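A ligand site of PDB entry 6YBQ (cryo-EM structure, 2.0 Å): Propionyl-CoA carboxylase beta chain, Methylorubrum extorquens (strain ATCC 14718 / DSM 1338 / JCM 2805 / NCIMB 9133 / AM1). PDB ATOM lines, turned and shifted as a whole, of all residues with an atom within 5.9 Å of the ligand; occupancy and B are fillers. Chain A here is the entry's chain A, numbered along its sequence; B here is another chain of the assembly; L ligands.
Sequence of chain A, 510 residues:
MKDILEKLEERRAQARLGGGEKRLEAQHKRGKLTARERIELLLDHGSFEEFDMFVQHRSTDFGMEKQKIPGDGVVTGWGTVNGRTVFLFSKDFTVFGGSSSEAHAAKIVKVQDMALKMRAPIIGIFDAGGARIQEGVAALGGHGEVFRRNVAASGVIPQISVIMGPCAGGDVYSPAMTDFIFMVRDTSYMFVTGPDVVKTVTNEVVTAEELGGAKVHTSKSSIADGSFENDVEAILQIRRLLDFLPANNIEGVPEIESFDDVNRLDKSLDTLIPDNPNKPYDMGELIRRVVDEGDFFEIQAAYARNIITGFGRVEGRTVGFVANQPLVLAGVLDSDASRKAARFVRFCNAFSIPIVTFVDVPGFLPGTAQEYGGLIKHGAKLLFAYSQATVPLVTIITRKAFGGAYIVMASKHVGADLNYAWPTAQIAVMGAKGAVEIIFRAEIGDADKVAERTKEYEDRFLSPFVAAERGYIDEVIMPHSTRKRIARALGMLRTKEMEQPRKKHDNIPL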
ATOM      1  N   ARG A  23     -11.545  16.226 -11.934  1.00  0.00           N
ATOM      2  CA  ARG A  23     -12.901  16.657 -12.232  1.00  0.00           C
ATOM      3  C   ARG A  23     -13.907  15.537 -11.974  1.00  0.00           C
ATOM      4  O   ARG A  23     -15.031  15.801 -11.532  1.00  0.00           O
ATOM      5  CB  ARG A  23     -12.985  17.134 -13.674  1.00  0.00           C
ATOM      6  CG  ARG A  23     -12.153  18.382 -13.971  1.00  0.00           C
ATOM      7  CD  ARG A  23     -12.432  18.914 -15.355  1.00  0.00           C
ATOM      8  NE  ARG A  23     -11.653  20.106 -15.679  1.00  0.00           N
ATOM      9  CZ  ARG A  23     -12.042  21.353 -15.438  1.00  0.00           C
ATOM     10  NH1 ARG A  23     -13.204  21.605 -14.860  1.00  0.00           N
ATOM     11  NH2 ARG A  23     -11.253  22.365 -15.770  1.00  0.00           N
ATOM     12  N   PHE A  93     -20.169  16.548 -18.149  1.00  0.00           N
ATOM     13  CA  PHE A  93     -19.939  17.861 -17.545  1.00  0.00           C
ATOM     14  C   PHE A  93     -18.466  18.185 -17.354  1.00  0.00           C
ATOM     15  O   PHE A  93     -18.114  19.362 -17.281  1.00  0.00           O
ATOM     16  CB  PHE A  93     -20.677  17.932 -16.205  1.00  0.00           C
ATOM     17  CG  PHE A  93     -20.715  19.310 -15.602  1.00  0.00           C
ATOM     18  CD1 PHE A  93     -21.492  20.302 -16.166  1.00  0.00           C
ATOM     19  CD2 PHE A  93     -20.001  19.603 -14.469  1.00  0.00           C
ATOM     20  CE1 PHE A  93     -21.535  21.560 -15.627  1.00  0.00           C
ATOM     21  CE2 PHE A  93     -20.042  20.860 -13.916  1.00  0.00           C
ATOM     22  CZ  PHE A  93     -20.812  21.843 -14.490  1.00  0.00           C
ATOM     23  N   PHE A  96     -15.407  20.742 -20.974  1.00  0.00           N
ATOM     24  CA  PHE A  96     -15.892  22.077 -21.335  1.00  0.00           C
ATOM     25  C   PHE A  96     -17.281  22.345 -20.748  1.00  0.00           C
ATOM     26  O   PHE A  96     -18.105  23.021 -21.363  1.00  0.00           O
ATOM     27  CB  PHE A  96     -15.907  22.257 -22.853  1.00  0.00           C
ATOM     28  CG  PHE A  96     -14.553  22.100 -23.499  1.00  0.00           C
ATOM     29  CD1 PHE A  96     -13.576  23.055 -23.337  1.00  0.00           C
ATOM     30  CD2 PHE A  96     -14.288  20.990 -24.287  1.00  0.00           C
ATOM     31  CE1 PHE A  96     -12.344  22.908 -23.923  1.00  0.00           C
ATOM     32  CE2 PHE A  96     -13.048  20.843 -24.890  1.00  0.00           C
ATOM     33  CZ  PHE A  96     -12.084  21.807 -24.702  1.00  0.00           C
ATOM     34  N   GLY A  97     -17.517  21.823 -19.550  1.00  0.00           N
ATOM     35  CA  GLY A  97     -18.808  22.021 -18.910  1.00  0.00           C
ATOM     36  C   GLY A  97     -19.964  21.431 -19.684  1.00  0.00           C
ATOM     37  O   GLY A  97     -21.083  21.960 -19.609  1.00  0.00           O
ATOM     38  N   GLY A  98     -19.733  20.351 -20.426  1.00  0.00           N
ATOM     39  CA  GLY A  98     -20.791  19.756 -21.226  1.00  0.00           C
ATOM     40  C   GLY A  98     -21.326  20.656 -22.317  1.00  0.00           C
ATOM     41  O   GLY A  98     -22.432  20.403 -22.814  1.00  0.00           O
ATOM     42  N   SER A  99     -20.588  21.679 -22.703  1.00  0.00           N
ATOM     43  CA  SER A  99     -21.091  22.657 -23.653  1.00  0.00           C
ATOM     44  C   SER A  99     -21.188  22.056 -25.059  1.00  0.00           C
ATOM     45  O   SER A  99     -20.521  21.080 -25.399  1.00  0.00           O
ATOM     46  CB  SER A  99     -20.199  23.900 -23.673  1.00  0.00           C
ATOM     47  OG  SER A  99     -18.887  23.584 -24.062  1.00  0.00           O
ATOM     48  N   ALA A 128     -25.009  20.131 -18.415  1.00  0.00           N
ATOM     49  CA  ALA A 128     -24.379  20.939 -19.450  1.00  0.00           C
ATOM     50  C   ALA A 128     -24.415  22.419 -19.067  1.00  0.00           C
ATOM     51  O   ALA A 128     -24.789  22.779 -17.949  1.00  0.00           O
ATOM     52  CB  ALA A 128     -25.069  20.703 -20.791  1.00  0.00           C
ATOM     53  N   GLY A 129     -23.986  23.265 -20.003  1.00  0.00           N
ATOM     54  CA  GLY A 129     -23.984  24.711 -19.841  1.00  0.00           C
ATOM     55  C   GLY A 129     -24.328  25.484 -21.105  1.00  0.00           C
ATOM     56  O   GLY A 129     -24.218  26.709 -21.126  1.00  0.00           O
ATOM     57  N   GLY A 130     -24.749  24.780 -22.159  1.00  0.00           N
ATOM     58  CA  GLY A 130     -25.226  25.448 -23.360  1.00  0.00           C
ATOM     59  C   GLY A 130     -24.243  25.492 -24.508  1.00  0.00           C
ATOM     60  O   GLY A 130     -23.350  24.648 -24.621  1.00  0.00           O
ATOM     61  N   ALA A 131     -24.405  26.489 -25.381  1.00  0.00           N
ATOM     62  CA  ALA A 131     -23.488  26.662 -26.509  1.00  0.00           C
ATOM     63  C   ALA A 131     -22.090  27.013 -26.018  1.00  0.00           C
ATOM     64  O   ALA A 131     -21.912  27.734 -25.032  1.00  0.00           O
ATOM     65  CB  ALA A 131     -24.002  27.768 -27.435  1.00  0.00           C
ATOM     66  N   ARG A 132     -21.087  26.491 -26.729  1.00  0.00           N
ATOM     67  CA  ARG A 132     -19.688  26.740 -26.388  1.00  0.00           C
ATOM     68  C   ARG A 132     -19.263  28.084 -26.975  1.00  0.00           C
ATOM     69  O   ARG A 132     -19.193  28.235 -28.208  1.00  0.00           O
ATOM     70  CB  ARG A 132     -18.803  25.605 -26.888  1.00  0.00           C
ATOM     71  CG  ARG A 132     -17.388  25.660 -26.370  1.00  0.00           C
ATOM     72  CD  ARG A 132     -16.549  24.477 -26.824  1.00  0.00           C
ATOM     73  NE  ARG A 132     -17.097  23.208 -26.365  1.00  0.00           N
ATOM     74  CZ  ARG A 132     -16.747  22.017 -26.852  1.00  0.00           C
ATOM     75  NH1 ARG A 132     -15.848  21.927 -27.826  1.00  0.00           N
ATOM     76  NH2 ARG A 132     -17.306  20.920 -26.377  1.00  0.00           N
ATOM     77  N   ILE A 133     -18.958  29.048 -26.107  1.00  0.00           N
ATOM     78  CA  ILE A 133     -18.787  30.428 -26.542  1.00  0.00           C
ATOM     79  C   ILE A 133     -17.593  30.566 -27.478  1.00  0.00           C
ATOM     80  O   ILE A 133     -17.655  31.283 -28.498  1.00  0.00           O
ATOM     81  CB  ILE A 133     -18.650  31.346 -25.315  1.00  0.00           C
ATOM     82  CG1 ILE A 133     -19.924  31.289 -24.463  1.00  0.00           C
ATOM     83  CG2 ILE A 133     -18.347  32.767 -25.733  1.00  0.00           C
ATOM     84  CD1 ILE A 133     -21.145  31.958 -25.084  1.00  0.00           C
ATOM     85  N   GLN A 134     -16.492  29.879 -27.185  1.00  0.00           N
ATOM     86  CA  GLN A 134     -15.270  30.036 -27.972  1.00  0.00           C
ATOM     87  C   GLN A 134     -15.504  29.717 -29.450  1.00  0.00           C
ATOM     88  O   GLN A 134     -14.788  30.244 -30.311  1.00  0.00           O
ATOM     89  CB  GLN A 134     -14.156  29.151 -27.414  1.00  0.00           C
ATOM     90  CG  GLN A 134     -13.680  29.537 -26.031  1.00  0.00           C
ATOM     91  CD  GLN A 134     -14.569  29.003 -24.937  1.00  0.00           C
ATOM     92  OE1 GLN A 134     -15.735  28.670 -25.165  1.00  0.00           O
ATOM     93  NE2 GLN A 134     -14.042  28.918 -23.727  1.00  0.00           N
ATOM     94  N   PRO A 166     -27.001  21.055 -14.309  1.00  0.00           N
ATOM     95  CA  PRO A 166     -27.405  22.337 -14.908  1.00  0.00           C
ATOM     96  C   PRO A 166     -27.847  22.159 -16.353  1.00  0.00           C
ATOM     97  O   PRO A 166     -27.372  21.286 -17.073  1.00  0.00           O
ATOM     98  CB  PRO A 166     -26.137  23.180 -14.828  1.00  0.00           C
ATOM     99  CG  PRO A 166     -25.309  22.565 -13.787  1.00  0.00           C
ATOM    100  CD  PRO A 166     -25.621  21.107 -13.799  1.00  0.00           C
ATOM    101  N   ALA A 168     -28.789  25.295 -19.104  1.00  0.00           N
ATOM    102  CA  ALA A 168     -28.980  26.722 -19.263  1.00  0.00           C
ATOM    103  C   ALA A 168     -28.870  27.120 -20.728  1.00  0.00           C
ATOM    104  O   ALA A 168     -28.160  26.484 -21.514  1.00  0.00           O
ATOM    105  CB  ALA A 168     -27.969  27.507 -18.432  1.00  0.00           C
ATOM    106  N   TYR A 189     -31.079  21.993 -12.413  1.00  0.00           N
ATOM    107  CA  TYR A 189     -31.903  23.176 -12.620  1.00  0.00           C
ATOM    108  C   TYR A 189     -31.959  23.529 -14.111  1.00  0.00           C
ATOM    109  O   TYR A 189     -31.132  23.095 -14.909  1.00  0.00           O
ATOM    110  CB  TYR A 189     -31.406  24.374 -11.812  1.00  0.00           C
ATOM    111  CG  TYR A 189     -29.930  24.672 -11.913  1.00  0.00           C
ATOM    112  CD1 TYR A 189     -29.421  25.406 -12.971  1.00  0.00           C
ATOM    113  CD2 TYR A 189     -29.035  24.262 -10.933  1.00  0.00           C
ATOM    114  CE1 TYR A 189     -28.076  25.691 -13.072  1.00  0.00           C
ATOM    115  CE2 TYR A 189     -27.700  24.542 -11.025  1.00  0.00           C
ATOM    116  CZ  TYR A 189     -27.217  25.262 -12.087  1.00  0.00           C
ATOM    117  OH  TYR A 189     -25.879  25.548 -12.172  1.00  0.00           O
ATOM    118  N   PHE A 191     -33.101  27.051 -16.772  1.00  0.00           N
ATOM    119  CA  PHE A 191     -33.578  28.402 -17.067  1.00  0.00           C
ATOM    120  C   PHE A 191     -32.932  28.894 -18.346  1.00  0.00           C
ATOM    121  O   PHE A 191     -31.860  28.443 -18.735  1.00  0.00           O
ATOM    122  CB  PHE A 191     -33.304  29.380 -15.924  1.00  0.00           C
ATOM    123  CG  PHE A 191     -31.970  29.193 -15.268  1.00  0.00           C
ATOM    124  CD1 PHE A 191     -30.801  29.521 -15.938  1.00  0.00           C
ATOM    125  CD2 PHE A 191     -31.875  28.686 -13.984  1.00  0.00           C
ATOM    126  CE1 PHE A 191     -29.582  29.349 -15.338  1.00  0.00           C
ATOM    127  CE2 PHE A 191     -30.656  28.513 -13.383  1.00  0.00           C
ATOM    128  CZ  PHE A 191     -29.509  28.849 -14.064  1.00  0.00           C
ATOM    129  N   ASP A 196     -26.944  36.110 -12.970  1.00  0.00           N
ATOM    130  CA  ASP A 196     -26.173  37.331 -13.122  1.00  0.00           C
ATOM    131  C   ASP A 196     -26.914  38.366 -13.971  1.00  0.00           C
ATOM    132  O   ASP A 196     -26.998  39.544 -13.607  1.00  0.00           O
ATOM    133  CB  ASP A 196     -24.802  37.011 -13.726  1.00  0.00           C
ATOM    134  CG  ASP A 196     -24.901  36.432 -15.122  1.00  0.00           C
ATOM    135  OD1 ASP A 196     -25.781  35.570 -15.349  1.00  0.00           O
ATOM    136  OD2 ASP A 196     -24.099  36.823 -15.993  1.00  0.00           O
ATOM    137  N   MET B 430     -23.462  36.349 -28.467  1.00  0.00           N
ATOM    138  CA  MET B 430     -23.876  37.356 -27.447  1.00  0.00           C
ATOM    139  C   MET B 430     -23.072  38.612 -27.738  1.00  0.00           C
ATOM    140  O   MET B 430     -22.217  38.679 -28.627  1.00  0.00           O
ATOM    141  CB  MET B 430     -23.635  36.964 -25.981  1.00  0.00           C
ATOM    142  CG  MET B 430     -22.183  36.695 -25.652  1.00  0.00           C
ATOM    143  SD  MET B 430     -21.873  36.603 -23.875  1.00  0.00           S
ATOM    144  CE  MET B 430     -22.543  34.976 -23.507  1.00  0.00           C
ATOM    145  N   ILE B 438     -16.598  36.291 -20.156  1.00  0.00           N
ATOM    146  CA  ILE B 438     -16.578  34.839 -19.969  1.00  0.00           C
ATOM    147  C   ILE B 438     -15.279  34.247 -20.497  1.00  0.00           C
ATOM    148  O   ILE B 438     -14.634  33.429 -19.836  1.00  0.00           O
ATOM    149  CB  ILE B 438     -17.809  34.189 -20.620  1.00  0.00           C
ATOM    150  CG1 ILE B 438     -19.087  34.780 -20.045  1.00  0.00           C
ATOM    151  CG2 ILE B 438     -17.770  32.687 -20.427  1.00  0.00           C
ATOM    152  CD1 ILE B 438     -20.334  34.447 -20.837  1.00  0.00           C
ATOM    153  N   ARG B 441     -11.590  35.487 -18.321  1.00  0.00           N
ATOM    154  CA  ARG B 441     -12.037  35.616 -16.942  1.00  0.00           C
ATOM    155  C   ARG B 441     -10.876  35.771 -15.966  1.00  0.00           C
ATOM    156  O   ARG B 441     -11.054  36.387 -14.912  1.00  0.00           O
ATOM    157  CB  ARG B 441     -12.890  34.405 -16.542  1.00  0.00           C
ATOM    158  CG  ARG B 441     -12.268  33.047 -16.838  1.00  0.00           C
ATOM    159  CD  ARG B 441     -13.263  31.923 -16.569  1.00  0.00           C
ATOM    160  NE  ARG B 441     -12.741  30.607 -16.936  1.00  0.00           N
ATOM    161  CZ  ARG B 441     -12.853  30.065 -18.152  1.00  0.00           C
ATOM    162  NH1 ARG B 441     -13.460  30.707 -19.136  1.00  0.00           N
ATOM    163  NH2 ARG B 441     -12.342  28.862 -18.374  1.00  0.00           N
HETATM  164  N1  LIG L   1     -19.147  27.665 -23.042  1.00  0.00           N
HETATM  165  C1  LIG L   1     -17.871  27.402 -22.694  1.00  0.00           C
HETATM  166  N2  LIG L   1     -17.387  26.971 -21.525  1.00  0.00           N
HETATM  167  C2  LIG L   1     -18.352  26.825 -20.602  1.00  0.00           C
HETATM  168  C3  LIG L   1     -19.694  27.046 -20.805  1.00  0.00           C
HETATM  169  C4  LIG L   1     -20.095  27.482 -22.084  1.00  0.00           C
HETATM  170  N3  LIG L   1     -21.355  27.729 -22.385  1.00  0.00           N
HETATM  171  N4  LIG L   1     -20.410  26.774 -19.647  1.00  0.00           N
HETATM  172  C5  LIG L   1     -19.498  26.404 -18.788  1.00  0.00           C
HETATM  173  N5  LIG L   1     -18.256  26.391 -19.310  1.00  0.00           N
HETATM  174  C6  LIG L   1     -17.107  26.080 -18.510  1.00  0.00           C
HETATM  175  C7  LIG L   1     -16.845  27.163 -17.462  1.00  0.00           C
HETATM  176  O1  LIG L   1     -16.119  28.238 -18.020  1.00  0.00           O
HETATM  177  C8  LIG L   1     -16.072  26.379 -16.408  1.00  0.00           C
HETATM  178  O2  LIG L   1     -14.734  26.173 -16.775  1.00  0.00           O
HETATM  179  P1  LIG L   1     -13.496  26.093 -15.726  1.00  0.00           P
HETATM  180  O3  LIG L   1     -13.266  27.419 -15.092  1.00  0.00           O
HETATM  181  O4  LIG L   1     -12.458  25.834 -16.666  1.00  0.00           O
HETATM  182  O5  LIG L   1     -13.606  25.022 -14.738  1.00  0.00           O
HETATM  183  C9  LIG L   1     -16.776  25.038 -16.421  1.00  0.00           C
HETATM  184  O6  LIG L   1     -17.412  24.969 -17.730  1.00  0.00           O
HETATM  185  C10 LIG L   1     -17.812  24.925 -15.329  1.00  0.00           C
HETATM  186  O7  LIG L   1     -18.594  26.168 -15.277  1.00  0.00           O
HETATM  187  P2  LIG L   1     -18.720  27.172 -14.057  1.00  0.00           P
HETATM  188  O8  LIG L   1     -19.538  28.343 -14.462  1.00  0.00           O
HETATM  189  O9  LIG L   1     -17.463  27.413 -13.386  1.00  0.00           O
HETATM  190  O10 LIG L   1     -19.571  26.334 -13.020  1.00  0.00           O
HETATM  191  P3  LIG L   1     -21.034  26.205 -12.351  1.00  0.00           P
HETATM  192  O11 LIG L   1     -21.337  24.806 -12.060  1.00  0.00           O
HETATM  193  O12 LIG L   1     -21.259  27.174 -11.290  1.00  0.00           O
HETATM  194  O13 LIG L   1     -22.059  26.763 -13.434  1.00  0.00           O
HETATM  195  C11 LIG L   1     -23.332  26.991 -15.516  1.00  0.00           C
HETATM  196  C12 LIG L   1     -22.547  26.041 -14.579  1.00  0.00           C
HETATM  197  C13 LIG L   1     -23.650  26.165 -16.764  1.00  0.00           C
HETATM  198  C14 LIG L   1     -24.672  27.339 -14.908  1.00  0.00           C
HETATM  199  C15 LIG L   1     -22.644  28.328 -15.958  1.00  0.00           C
HETATM  200  O14 LIG L   1     -21.336  28.147 -16.345  1.00  0.00           O
HETATM  201  C16 LIG L   1     -23.356  29.026 -17.105  1.00  0.00           C
HETATM  202  O15 LIG L   1     -24.359  29.659 -16.880  1.00  0.00           O
HETATM  203  N6  LIG L   1     -22.872  28.906 -18.331  1.00  0.00           N
HETATM  204  C17 LIG L   1     -23.448  29.398 -19.563  1.00  0.00           C
HETATM  205  C18 LIG L   1     -22.679  30.594 -20.130  1.00  0.00           C
HETATM  206  C19 LIG L   1     -22.686  31.803 -19.212  1.00  0.00           C
HETATM  207  O16 LIG L   1     -23.459  32.732 -19.387  1.00  0.00           O
HETATM  208  N7  LIG L   1     -21.785  31.890 -18.269  1.00  0.00           N
HETATM  209  C20 LIG L   1     -21.729  33.085 -17.437  1.00  0.00           C
HETATM  210  C21 LIG L   1     -22.401  32.915 -16.108  1.00  0.00           C
HETATM  211  S1  LIG L   1     -21.690  31.625 -15.067  1.00  0.00           S
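A nitrogen (N3) of the ligand is in hydrogen-bond range of the backbone carbonyl oxygen (O) of Ala 131 (2.7 Å). The backbone carbonyl oxygen of Gly 129 lies close to a nitrogen (N3) of the ligand, 3.3 Å away. The backbone NH (N) of Ile 133 lies within hydrogen-bond range of a nitrogen (N1) of the ligand, 3.4 Å away. NH1 of Arg 23 is in salt-bridge range of O5 of the ligand. An oxygen (O4) of the ligand lies within salt-bridge range of the guanidinium group of Arg 441 of chain B, at 3.5 Å.
O of Gly 97 sits at hydrogen-bond distance from N of Gly 129 (3.2 Å). The backbone carbonyl oxygen (O) of Ile 438 of chain B sits at hydrogen-bond distance from the guanidinium group (NH1) of Arg 441 of chain B (3.0 Å). The guanidinium group (NE) of Arg 132 sits at hydrogen-bond distance from the side-chain hydroxyl (OG) of Ser 99 (2.9 Å). The backbone NH of Ala 128 lies within hydrogen-bond range of the backbone carbonyl oxygen of Pro 166, 3.0 Å away. The side-chain hydroxyl (OG) of Ser 99 is in hydrogen-bond range of the backbone carbonyl oxygen (O) of Phe 96 (2.9 Å).
Residues that only touch the ligand: Phe 93 (3.9 Å), Phe 96 (3.9 Å), Gly 97 (3.5 Å), Ser 99 (3.9 Å), Ala 128 (3.8 Å), Arg 132 (3.5 Å), Gln 134 (3.5 Å), Tyr 189 (3.5 Å) and Ile 438 of chain B (3.8 Å). Of the 21 residues printed, 14 come within 4 Å of the ligand.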
